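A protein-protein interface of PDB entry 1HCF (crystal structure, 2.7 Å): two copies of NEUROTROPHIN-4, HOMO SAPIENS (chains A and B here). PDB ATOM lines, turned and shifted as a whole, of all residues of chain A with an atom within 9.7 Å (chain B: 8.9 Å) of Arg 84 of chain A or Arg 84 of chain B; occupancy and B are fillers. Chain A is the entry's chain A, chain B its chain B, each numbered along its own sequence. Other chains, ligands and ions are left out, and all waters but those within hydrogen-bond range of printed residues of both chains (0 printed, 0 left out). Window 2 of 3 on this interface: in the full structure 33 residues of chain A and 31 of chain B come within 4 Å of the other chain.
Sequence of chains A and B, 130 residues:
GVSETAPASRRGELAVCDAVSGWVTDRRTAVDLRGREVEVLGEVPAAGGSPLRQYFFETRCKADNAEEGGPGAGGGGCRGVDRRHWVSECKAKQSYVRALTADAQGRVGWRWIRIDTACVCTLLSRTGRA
The backbone carbonyl oxygen (O) of Gly 80 of chain A is in hydrogen-bond range of the backbone NH (N) of Asp 82 of chain B, at 2.8 Å. The backbone NH (N) of Asp 82 of chain A sits at hydrogen-bond distance from the backbone carbonyl oxygen (O) of Gly 80 of chain B, at 2.8 Å. The side-chain carboxylate (OD2) of Asp 82 of chain A sits close to the side-chain carboxylate (OD2) of Asp 82 of chain B (3.4 Å). NH1 of Arg 84 of chain A sits close to NH1 of Arg 84 of chain B.
The side-chain carboxylate of Asp 82 of chain A is in salt-bridge range of the guanidinium group of Arg 84 of chain A (3.2 Å). O of Trp 86 of chain A sits at hydrogen-bond distance from NE of Arg 126 of chain A, at 3.3 Å. OD2 of Asp 82 of chain B lies within salt-bridge range of NH2 of Arg 84 of chain B. The guanidinium group (NH1) of Arg 126 of chain B sits at hydrogen-bond distance from the backbone carbonyl oxygen (O) of Arg 84 of chain B, 3.0 Å away.
Among the printed residues, merely in contact across the chains: Gly 80 of chain A with Val 81 of chain B (3.1 Å), Val 81 of chain A with Gly 80 of chain B (3.3 Å), Trp 86 of chain A with Gly 80 of chain B (3.5 Å) and Gly 80 of chain A with Trp 86 of chain B (3.5 Å).
Of chain B, only Arg 84 comes within 4 Å of Arg 84 of chain A. Of the printed residues of chain A, Arg 84 of chain B touches Arg 84. Asp 82 of chain B touches just these residues of chain A: Gly 80 and Asp 82. No residue of chain A comes within 4 Å of His 85 of chain B. Of the printed residues of chain B, Gly 80 of chain A touches Val 81 (3.1 Å), Asp 82 (2.8 Å) and Trp 86 (3.5 Å). Printed residues of chain B within 4 Å of Trp 86 of chain A: Gly 80. Of the printed residues of chain B, Val 81 of chain A touches Gly 80. The nearest residue of chain A that does not touch Arg 84 of chain B is Asp 82 of chain A (4.5 Å).
Of the 13 printed residues of chain B, 5 touch a printed residue of chain A. Hydrophobic or aromatic side chains of chain B within 4 Å of the printed part of chain A: Val 81 and Trp 86. Of the 13 printed residues of chain A, 5 touch a printed residue of chain B. Printed residues of chain A that touch a printed residue of chain B: Gly 80, Val 81, Asp 82, Arg 84 and Trp 86. Among the printed residues, 8 pairs touch across the chains. Among the printed residues, no Asp or Glu carboxylate lies within 4 Å of a Lys or Arg side-chain nitrogen of the other chain.
Gly 80 of chain A touches Asp 82 of chain B, and with the chains exchanged Asp 82 of chain A touches Gly 80 of chain B. Gly 80 of chain A touches Trp 86 of chain B, and with the chains exchanged Trp 86 of chain A touches Gly 80 of chain B. Asp 82 of chain B touches its own counterpart, Asp 82 of chain A. Arg 84 of chain B touches its own counterpart, Arg 84 of chain A. 12 positions are printed for both chains. Of the 8 pairs that touch across the chains among the printed residues, 8 have their exchanged pair printed and touching as well.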
ATOM      1  N   GLY A  80     -17.893 -20.606  -7.995  1.00  0.00           N
ATOM      2  CA  GLY A  80     -17.670 -22.001  -8.341  1.00  0.00           C
ATOM      3  C   GLY A  80     -16.560 -22.273  -9.342  1.00  0.00           C
ATOM      4  O   GLY A  80     -16.179 -23.424  -9.548  1.00  0.00           O
ATOM      5  N   VAL A  81     -16.043 -21.231  -9.982  1.00  0.00           N
ATOM      6  CA  VAL A  81     -14.969 -21.429 -10.939  1.00  0.00           C
ATOM      7  C   VAL A  81     -13.662 -21.635 -10.199  1.00  0.00           C
ATOM      8  O   VAL A  81     -13.408 -20.983  -9.182  1.00  0.00           O
ATOM      9  CB  VAL A  81     -14.808 -20.231 -11.890  1.00  0.00           C
ATOM     10  CG1 VAL A  81     -13.462 -20.315 -12.610  1.00  0.00           C
ATOM     11  CG2 VAL A  81     -15.920 -20.243 -12.914  1.00  0.00           C
ATOM     12  N   ASP A  82     -12.840 -22.541 -10.721  1.00  0.00           N
ATOM     13  CA  ASP A  82     -11.548 -22.857 -10.130  1.00  0.00           C
ATOM     14  C   ASP A  82     -10.504 -21.815 -10.531  1.00  0.00           C
ATOM     15  O   ASP A  82      -9.934 -21.893 -11.623  1.00  0.00           O
ATOM     16  CB  ASP A  82     -11.089 -24.244 -10.594  1.00  0.00           C
ATOM     17  CG  ASP A  82      -9.920 -24.790  -9.774  1.00  0.00           C
ATOM     18  OD1 ASP A  82      -9.032 -24.002  -9.373  1.00  0.00           O
ATOM     19  OD2 ASP A  82      -9.884 -26.017  -9.543  1.00  0.00           O
ATOM     20  N   ARG A  83     -10.253 -20.851  -9.646  1.00  0.00           N
ATOM     21  CA  ARG A  83      -9.272 -19.795  -9.899  1.00  0.00           C
ATOM     22  C   ARG A  83      -7.854 -20.297 -10.151  1.00  0.00           C
ATOM     23  O   ARG A  83      -7.058 -19.612 -10.798  1.00  0.00           O
ATOM     24  CB  ARG A  83      -9.243 -18.801  -8.735  1.00  0.00           C
ATOM     25  CG  ARG A  83     -10.326 -17.730  -8.800  1.00  0.00           C
ATOM     26  CD  ARG A  83     -10.295 -16.801  -7.598  1.00  0.00           C
ATOM     27  N   ARG A  84      -7.531 -21.483  -9.644  1.00  0.00           N
ATOM     28  CA  ARG A  84      -6.190 -22.037  -9.832  1.00  0.00           C
ATOM     29  C   ARG A  84      -5.841 -22.196 -11.311  1.00  0.00           C
ATOM     30  O   ARG A  84      -4.676 -22.115 -11.693  1.00  0.00           O
ATOM     31  CB  ARG A  84      -6.055 -23.412  -9.164  1.00  0.00           C
ATOM     32  CG  ARG A  84      -6.224 -23.451  -7.653  1.00  0.00           C
ATOM     33  CD  ARG A  84      -6.017 -24.878  -7.135  1.00  0.00           C
ATOM     34  NE  ARG A  84      -6.865 -25.841  -7.836  1.00  0.00           N
ATOM     35  CZ  ARG A  84      -6.848 -27.157  -7.640  1.00  0.00           C
ATOM     36  NH1 ARG A  84      -6.021 -27.703  -6.756  1.00  0.00           N
ATOM     37  NH2 ARG A  84      -7.668 -27.933  -8.333  1.00  0.00           N
ATOM     38  N   HIS A  85      -6.851 -22.421 -12.142  1.00  0.00           N
ATOM     39  CA  HIS A  85      -6.608 -22.632 -13.559  1.00  0.00           C
ATOM     40  C   HIS A  85      -7.385 -21.713 -14.489  1.00  0.00           C
ATOM     41  O   HIS A  85      -7.171 -21.748 -15.702  1.00  0.00           O
ATOM     42  CB  HIS A  85      -6.939 -24.081 -13.916  1.00  0.00           C
ATOM     43  CG  HIS A  85      -6.242 -25.089 -13.056  1.00  0.00           C
ATOM     44  ND1 HIS A  85      -6.825 -26.285 -12.692  1.00  0.00           N
ATOM     45  CD2 HIS A  85      -5.015 -25.076 -12.481  1.00  0.00           C
ATOM     46  CE1 HIS A  85      -5.987 -26.964 -11.928  1.00  0.00           C
ATOM     47  NE2 HIS A  85      -4.883 -26.253 -11.786  1.00  0.00           N
ATOM     48  N   TRP A  86      -8.279 -20.889 -13.941  1.00  0.00           N
ATOM     49  CA  TRP A  86      -9.077 -20.020 -14.797  1.00  0.00           C
ATOM     50  C   TRP A  86      -9.260 -18.574 -14.387  1.00  0.00           C
ATOM     51  O   TRP A  86      -9.146 -18.201 -13.220  1.00  0.00           O
ATOM     52  CB  TRP A  86     -10.475 -20.609 -15.007  1.00  0.00           C
ATOM     53  CG  TRP A  86     -10.501 -22.004 -15.545  1.00  0.00           C
ATOM     54  CD1 TRP A  86     -10.637 -23.154 -14.826  1.00  0.00           C
ATOM     55  CD2 TRP A  86     -10.404 -22.396 -16.919  1.00  0.00           C
ATOM     56  NE1 TRP A  86     -10.637 -24.241 -15.667  1.00  0.00           N
ATOM     57  CE2 TRP A  86     -10.494 -23.807 -16.958  1.00  0.00           C
ATOM     58  CE3 TRP A  86     -10.248 -21.693 -18.126  1.00  0.00           C
ATOM     59  CZ2 TRP A  86     -10.436 -24.534 -18.158  1.00  0.00           C
ATOM     60  CZ3 TRP A  86     -10.190 -22.417 -19.324  1.00  0.00           C
ATOM     61  CH2 TRP A  86     -10.284 -23.825 -19.325  1.00  0.00           C
ATOM     62  N   VAL A  87      -9.556 -17.771 -15.400  1.00  0.00           N
ATOM     63  CA  VAL A  87      -9.838 -16.360 -15.255  1.00  0.00           C
ATOM     64  C   VAL A  87     -11.257 -16.317 -15.806  1.00  0.00           C
ATOM     65  O   VAL A  87     -11.483 -16.610 -16.987  1.00  0.00           O
ATOM     66  CB  VAL A  87      -8.923 -15.508 -16.138  1.00  0.00           C
ATOM     67  CG1 VAL A  87      -9.291 -14.036 -15.993  1.00  0.00           C
ATOM     68  CG2 VAL A  87      -7.475 -15.742 -15.754  1.00  0.00           C
ATOM     69  N   SER A  88     -12.210 -15.984 -14.943  1.00  0.00           N
ATOM     70  CA  SER A  88     -13.609 -15.947 -15.326  1.00  0.00           C
ATOM     71  C   SER A  88     -14.253 -14.588 -15.131  1.00  0.00           C
ATOM     72  O   SER A  88     -13.809 -13.777 -14.317  1.00  0.00           O
ATOM     73  CB  SER A  88     -14.388 -16.987 -14.519  1.00  0.00           C
ATOM     74  OG  SER A  88     -14.450 -16.632 -13.144  1.00  0.00           O
ATOM     75  N   LEU A 124     -11.111 -18.347 -19.305  1.00  0.00           N
ATOM     76  CA  LEU A 124      -9.813 -18.200 -19.959  1.00  0.00           C
ATOM     77  C   LEU A 124      -8.780 -18.903 -19.092  1.00  0.00           C
ATOM     78  O   LEU A 124      -8.665 -18.619 -17.898  1.00  0.00           O
ATOM     79  CB  LEU A 124      -9.429 -16.728 -20.121  1.00  0.00           C
ATOM     80  CG  LEU A 124     -10.018 -16.055 -21.355  1.00  0.00           C
ATOM     81  CD1 LEU A 124      -9.647 -14.595 -21.367  1.00  0.00           C
ATOM     82  CD2 LEU A 124      -9.507 -16.763 -22.607  1.00  0.00           C
ATOM     83  N   SER A 125      -8.044 -19.834 -19.690  1.00  0.00           N
ATOM     84  CA  SER A 125      -7.014 -20.563 -18.963  1.00  0.00           C
ATOM     85  C   SER A 125      -5.948 -19.573 -18.497  1.00  0.00           C
ATOM     86  O   SER A 125      -5.523 -18.718 -19.271  1.00  0.00           O
ATOM     87  CB  SER A 125      -6.389 -21.623 -19.867  1.00  0.00           C
ATOM     88  OG  SER A 125      -5.471 -22.424 -19.145  1.00  0.00           O
ATOM     89  N   ARG A 126      -5.530 -19.688 -17.236  1.00  0.00           N
ATOM     90  CA  ARG A 126      -4.525 -18.792 -16.649  1.00  0.00           C
ATOM     91  C   ARG A 126      -3.339 -18.489 -17.562  1.00  0.00           C
ATOM     92  O   ARG A 126      -3.099 -17.332 -17.925  1.00  0.00           O
ATOM     93  CB  ARG A 126      -3.992 -19.370 -15.332  1.00  0.00           C
ATOM     94  CG  ARG A 126      -4.930 -19.236 -14.138  1.00  0.00           C
ATOM     95  CD  ARG A 126      -4.998 -17.810 -13.605  1.00  0.00           C
ATOM     96  NE  ARG A 126      -5.996 -17.686 -12.542  1.00  0.00           N
ATOM     97  CZ  ARG A 126      -6.293 -16.555 -11.906  1.00  0.00           C
ATOM     98  NH1 ARG A 126      -5.665 -15.427 -12.216  1.00  0.00           N
ATOM     99  NH2 ARG A 126      -7.231 -16.551 -10.967  1.00  0.00           N
ATOM    100  N   THR A 127      -2.592 -19.531 -17.917  1.00  0.00           N
ATOM    101  CA  THR A 127      -1.428 -19.379 -18.785  1.00  0.00           C
ATOM    102  C   THR A 127      -1.859 -19.322 -20.250  1.00  0.00           C
ATOM    103  O   THR A 127      -0.967 -19.132 -21.103  1.00  0.00           O
ATOM    104  CB  THR A 127      -0.433 -20.554 -18.590  1.00  0.00           C
ATOM    105  OG1 THR A 127       0.757 -20.309 -19.352  1.00  0.00           O
ATOM    106  CG2 THR A 127      -1.066 -21.873 -19.042  1.00  0.00           C
ATOM    107  N   GLY B  80     -14.716 -25.656 -16.070  1.00  0.00           N
ATOM    108  CA  GLY B  80     -14.066 -24.718 -15.170  1.00  0.00           C
ATOM    109  C   GLY B  80     -14.501 -24.645 -13.716  1.00  0.00           C
ATOM    110  O   GLY B  80     -13.942 -23.867 -12.941  1.00  0.00           O
ATOM    111  N   VAL B  81     -15.490 -25.442 -13.335  1.00  0.00           N
ATOM    112  CA  VAL B  81     -15.972 -25.428 -11.958  1.00  0.00           C
ATOM    113  C   VAL B  81     -15.070 -26.269 -11.071  1.00  0.00           C
ATOM    114  O   VAL B  81     -14.609 -27.333 -11.477  1.00  0.00           O
ATOM    115  CB  VAL B  81     -17.403 -25.989 -11.862  1.00  0.00           C
ATOM    116  CG1 VAL B  81     -17.804 -26.144 -10.395  1.00  0.00           C
ATOM    117  CG2 VAL B  81     -18.371 -25.070 -12.599  1.00  0.00           C
ATOM    118  N   ASP B  82     -14.825 -25.799  -9.854  1.00  0.00           N
ATOM    119  CA  ASP B  82     -13.973 -26.537  -8.938  1.00  0.00           C
ATOM    120  C   ASP B  82     -14.729 -27.693  -8.299  1.00  0.00           C
ATOM    121  O   ASP B  82     -15.498 -27.495  -7.363  1.00  0.00           O
ATOM    122  CB  ASP B  82     -13.442 -25.630  -7.834  1.00  0.00           C
ATOM    123  CG  ASP B  82     -12.191 -26.193  -7.177  1.00  0.00           C
ATOM    124  OD1 ASP B  82     -11.968 -27.429  -7.255  1.00  0.00           O
ATOM    125  OD2 ASP B  82     -11.435 -25.397  -6.584  1.00  0.00           O
ATOM    126  N   ARG B  83     -14.493 -28.900  -8.804  1.00  0.00           N
ATOM    127  CA  ARG B  83     -15.158 -30.088  -8.287  1.00  0.00           C
ATOM    128  C   ARG B  83     -14.788 -30.434  -6.846  1.00  0.00           C
ATOM    129  O   ARG B  83     -15.481 -31.216  -6.191  1.00  0.00           O
ATOM    130  CB  ARG B  83     -14.891 -31.274  -9.214  1.00  0.00           C
ATOM    131  CG  ARG B  83     -15.754 -31.236 -10.456  1.00  0.00           C
ATOM    132  CD  ARG B  83     -14.982 -31.489 -11.743  1.00  0.00           C
ATOM    133  NE  ARG B  83     -14.902 -32.899 -12.120  1.00  0.00           N
ATOM    134  CZ  ARG B  83     -15.926 -33.751 -12.102  1.00  0.00           C
ATOM    135  NH1 ARG B  83     -17.133 -33.358 -11.709  1.00  0.00           N
ATOM    136  NH2 ARG B  83     -15.746 -35.001 -12.513  1.00  0.00           N
ATOM    137  N   ARG B  84     -13.710 -29.851  -6.341  1.00  0.00           N
ATOM    138  CA  ARG B  84     -13.318 -30.124  -4.967  1.00  0.00           C
ATOM    139  C   ARG B  84     -14.379 -29.598  -4.004  1.00  0.00           C
ATOM    140  O   ARG B  84     -14.561 -30.131  -2.910  1.00  0.00           O
ATOM    141  CB  ARG B  84     -11.984 -29.448  -4.631  1.00  0.00           C
ATOM    142  CG  ARG B  84     -10.793 -29.985  -5.391  1.00  0.00           C
ATOM    143  CD  ARG B  84      -9.531 -29.262  -4.976  1.00  0.00           C
ATOM    144  NE  ARG B  84      -9.629 -27.828  -5.214  1.00  0.00           N
ATOM    145  CZ  ARG B  84      -8.662 -26.958  -4.942  1.00  0.00           C
ATOM    146  NH1 ARG B  84      -7.513 -27.376  -4.417  1.00  0.00           N
ATOM    147  NH2 ARG B  84      -8.841 -25.668  -5.193  1.00  0.00           N
ATOM    148  N   HIS B  85     -15.090 -28.557  -4.414  1.00  0.00           N
ATOM    149  CA  HIS B  85     -16.080 -27.963  -3.534  1.00  0.00           C
ATOM    150  C   HIS B  85     -17.472 -27.845  -4.113  1.00  0.00           C
ATOM    151  O   HIS B  85     -18.424 -27.575  -3.379  1.00  0.00           O
ATOM    152  CB  HIS B  85     -15.597 -26.580  -3.112  1.00  0.00           C
ATOM    153  CG  HIS B  85     -14.195 -26.574  -2.590  1.00  0.00           C
ATOM    154  ND1 HIS B  85     -13.240 -25.682  -3.031  1.00  0.00           N
ATOM    155  CD2 HIS B  85     -13.578 -27.365  -1.678  1.00  0.00           C
ATOM    156  CE1 HIS B  85     -12.097 -25.926  -2.414  1.00  0.00           C
ATOM    157  NE2 HIS B  85     -12.276 -26.940  -1.589  1.00  0.00           N
ATOM    158  N   TRP B  86     -17.606 -28.044  -5.419  1.00  0.00           N
ATOM    159  CA  TRP B  86     -18.914 -27.914  -6.027  1.00  0.00           C
ATOM    160  C   TRP B  86     -19.323 -29.015  -6.978  1.00  0.00           C
ATOM    161  O   TRP B  86     -18.492 -29.663  -7.610  1.00  0.00           O
ATOM    162  CB  TRP B  86     -19.026 -26.600  -6.790  1.00  0.00           C
ATOM    163  CG  TRP B  86     -18.603 -25.400  -6.041  1.00  0.00           C
ATOM    164  CD1 TRP B  86     -17.366 -24.825  -6.043  1.00  0.00           C
ATOM    165  CD2 TRP B  86     -19.429 -24.578  -5.204  1.00  0.00           C
ATOM    166  NE1 TRP B  86     -17.371 -23.690  -5.267  1.00  0.00           N
ATOM    167  CE2 TRP B  86     -18.624 -23.515  -4.740  1.00  0.00           C
ATOM    168  CE3 TRP B  86     -20.775 -24.637  -4.806  1.00  0.00           C
ATOM    169  CZ2 TRP B  86     -19.119 -22.512  -3.896  1.00  0.00           C
ATOM    170  CZ3 TRP B  86     -21.268 -23.634  -3.963  1.00  0.00           C
ATOM    171  CH2 TRP B  86     -20.439 -22.588  -3.521  1.00  0.00           C
ATOM    172  N   VAL B  87     -20.635 -29.202  -7.058  1.00  0.00           N
ATOM    173  CA  VAL B  87     -21.263 -30.151  -7.954  1.00  0.00           C
ATOM    174  C   VAL B  87     -22.079 -29.209  -8.825  1.00  0.00           C
ATOM    175  O   VAL B  87     -22.944 -28.481  -8.326  1.00  0.00           O
ATOM    176  CB  VAL B  87     -22.203 -31.098  -7.199  1.00  0.00           C
ATOM    177  CG1 VAL B  87     -23.301 -31.572  -8.114  1.00  0.00           C
ATOM    178  CG2 VAL B  87     -21.427 -32.284  -6.685  1.00  0.00           C
ATOM    179  N   LEU B 124     -23.959 -26.538  -6.316  1.00  0.00           N
ATOM    180  CA  LEU B 124     -24.394 -27.282  -5.130  1.00  0.00           C
ATOM    181  C   LEU B 124     -23.120 -27.617  -4.352  1.00  0.00           C
ATOM    182  O   LEU B 124     -22.309 -28.434  -4.794  1.00  0.00           O
ATOM    183  CB  LEU B 124     -25.120 -28.564  -5.516  1.00  0.00           C
ATOM    184  CG  LEU B 124     -26.566 -28.386  -5.959  1.00  0.00           C
ATOM    185  CD1 LEU B 124     -27.110 -29.698  -6.492  1.00  0.00           C
ATOM    186  CD2 LEU B 124     -27.385 -27.894  -4.787  1.00  0.00           C
ATOM    187  N   SER B 125     -22.938 -26.971  -3.202  1.00  0.00           N
ATOM    188  CA  SER B 125     -21.752 -27.186  -2.378  1.00  0.00           C
ATOM    189  C   SER B 125     -21.558 -28.633  -1.982  1.00  0.00           C
ATOM    190  O   SER B 125     -22.506 -29.410  -1.927  1.00  0.00           O
ATOM    191  CB  SER B 125     -21.806 -26.325  -1.117  1.00  0.00           C
ATOM    192  OG  SER B 125     -20.568 -26.370  -0.426  1.00  0.00           O
ATOM    193  N   ARG B 126     -20.308 -28.972  -1.696  1.00  0.00           N
ATOM    194  CA  ARG B 126     -19.902 -30.320  -1.314  1.00  0.00           C
ATOM    195  C   ARG B 126     -18.606 -30.150  -0.522  1.00  0.00           C
ATOM    196  O   ARG B 126     -18.031 -31.113  -0.009  1.00  0.00           O
ATOM    197  CB  ARG B 126     -19.662 -31.150  -2.584  1.00  0.00           C
ATOM    198  CG  ARG B 126     -18.638 -32.277  -2.467  1.00  0.00           C
ATOM    199  CD  ARG B 126     -17.760 -32.346  -3.727  1.00  0.00           C
ATOM    200  NE  ARG B 126     -16.654 -33.304  -3.619  1.00  0.00           N
ATOM    201  CZ  ARG B 126     -15.776 -33.341  -2.615  1.00  0.00           C
ATOM    202  NH1 ARG B 126     -15.864 -32.480  -1.608  1.00  0.00           N
ATOM    203  NH2 ARG B 126     -14.789 -34.230  -2.629  1.00  0.00           N
ATOM    204  N   THR B 127     -18.177 -28.894  -0.427  1.00  0.00           N
ATOM    205  CA  THR B 127     -16.956 -28.492   0.264  1.00  0.00           C
ATOM    206  C   THR B 127     -16.789 -29.118   1.640  1.00  0.00           C
ATOM    207  O   THR B 127     -17.691 -29.787   2.149  1.00  0.00           O
ATOM    208  CB  THR B 127     -16.913 -26.961   0.449  1.00  0.00           C
ATOM    209  OG1 THR B 127     -17.420 -26.320  -0.730  1.00  0.00           O
ATOM    210  CG2 THR B 127     -15.480 -26.492   0.707  1.00  0.00           C
ATOM    211  N   GLY B 128     -15.627 -28.874   2.243  1.00  0.00           N
ATOM    212  CA  GLY B 128     -15.343 -29.401   3.561  1.00  0.00           C
ATOM    213  C   GLY B 128     -15.132 -28.289   4.562  1.00  0.00           C
ATOM    214  O   GLY B 128     -15.179 -28.591   5.770  1.00  0.00           O
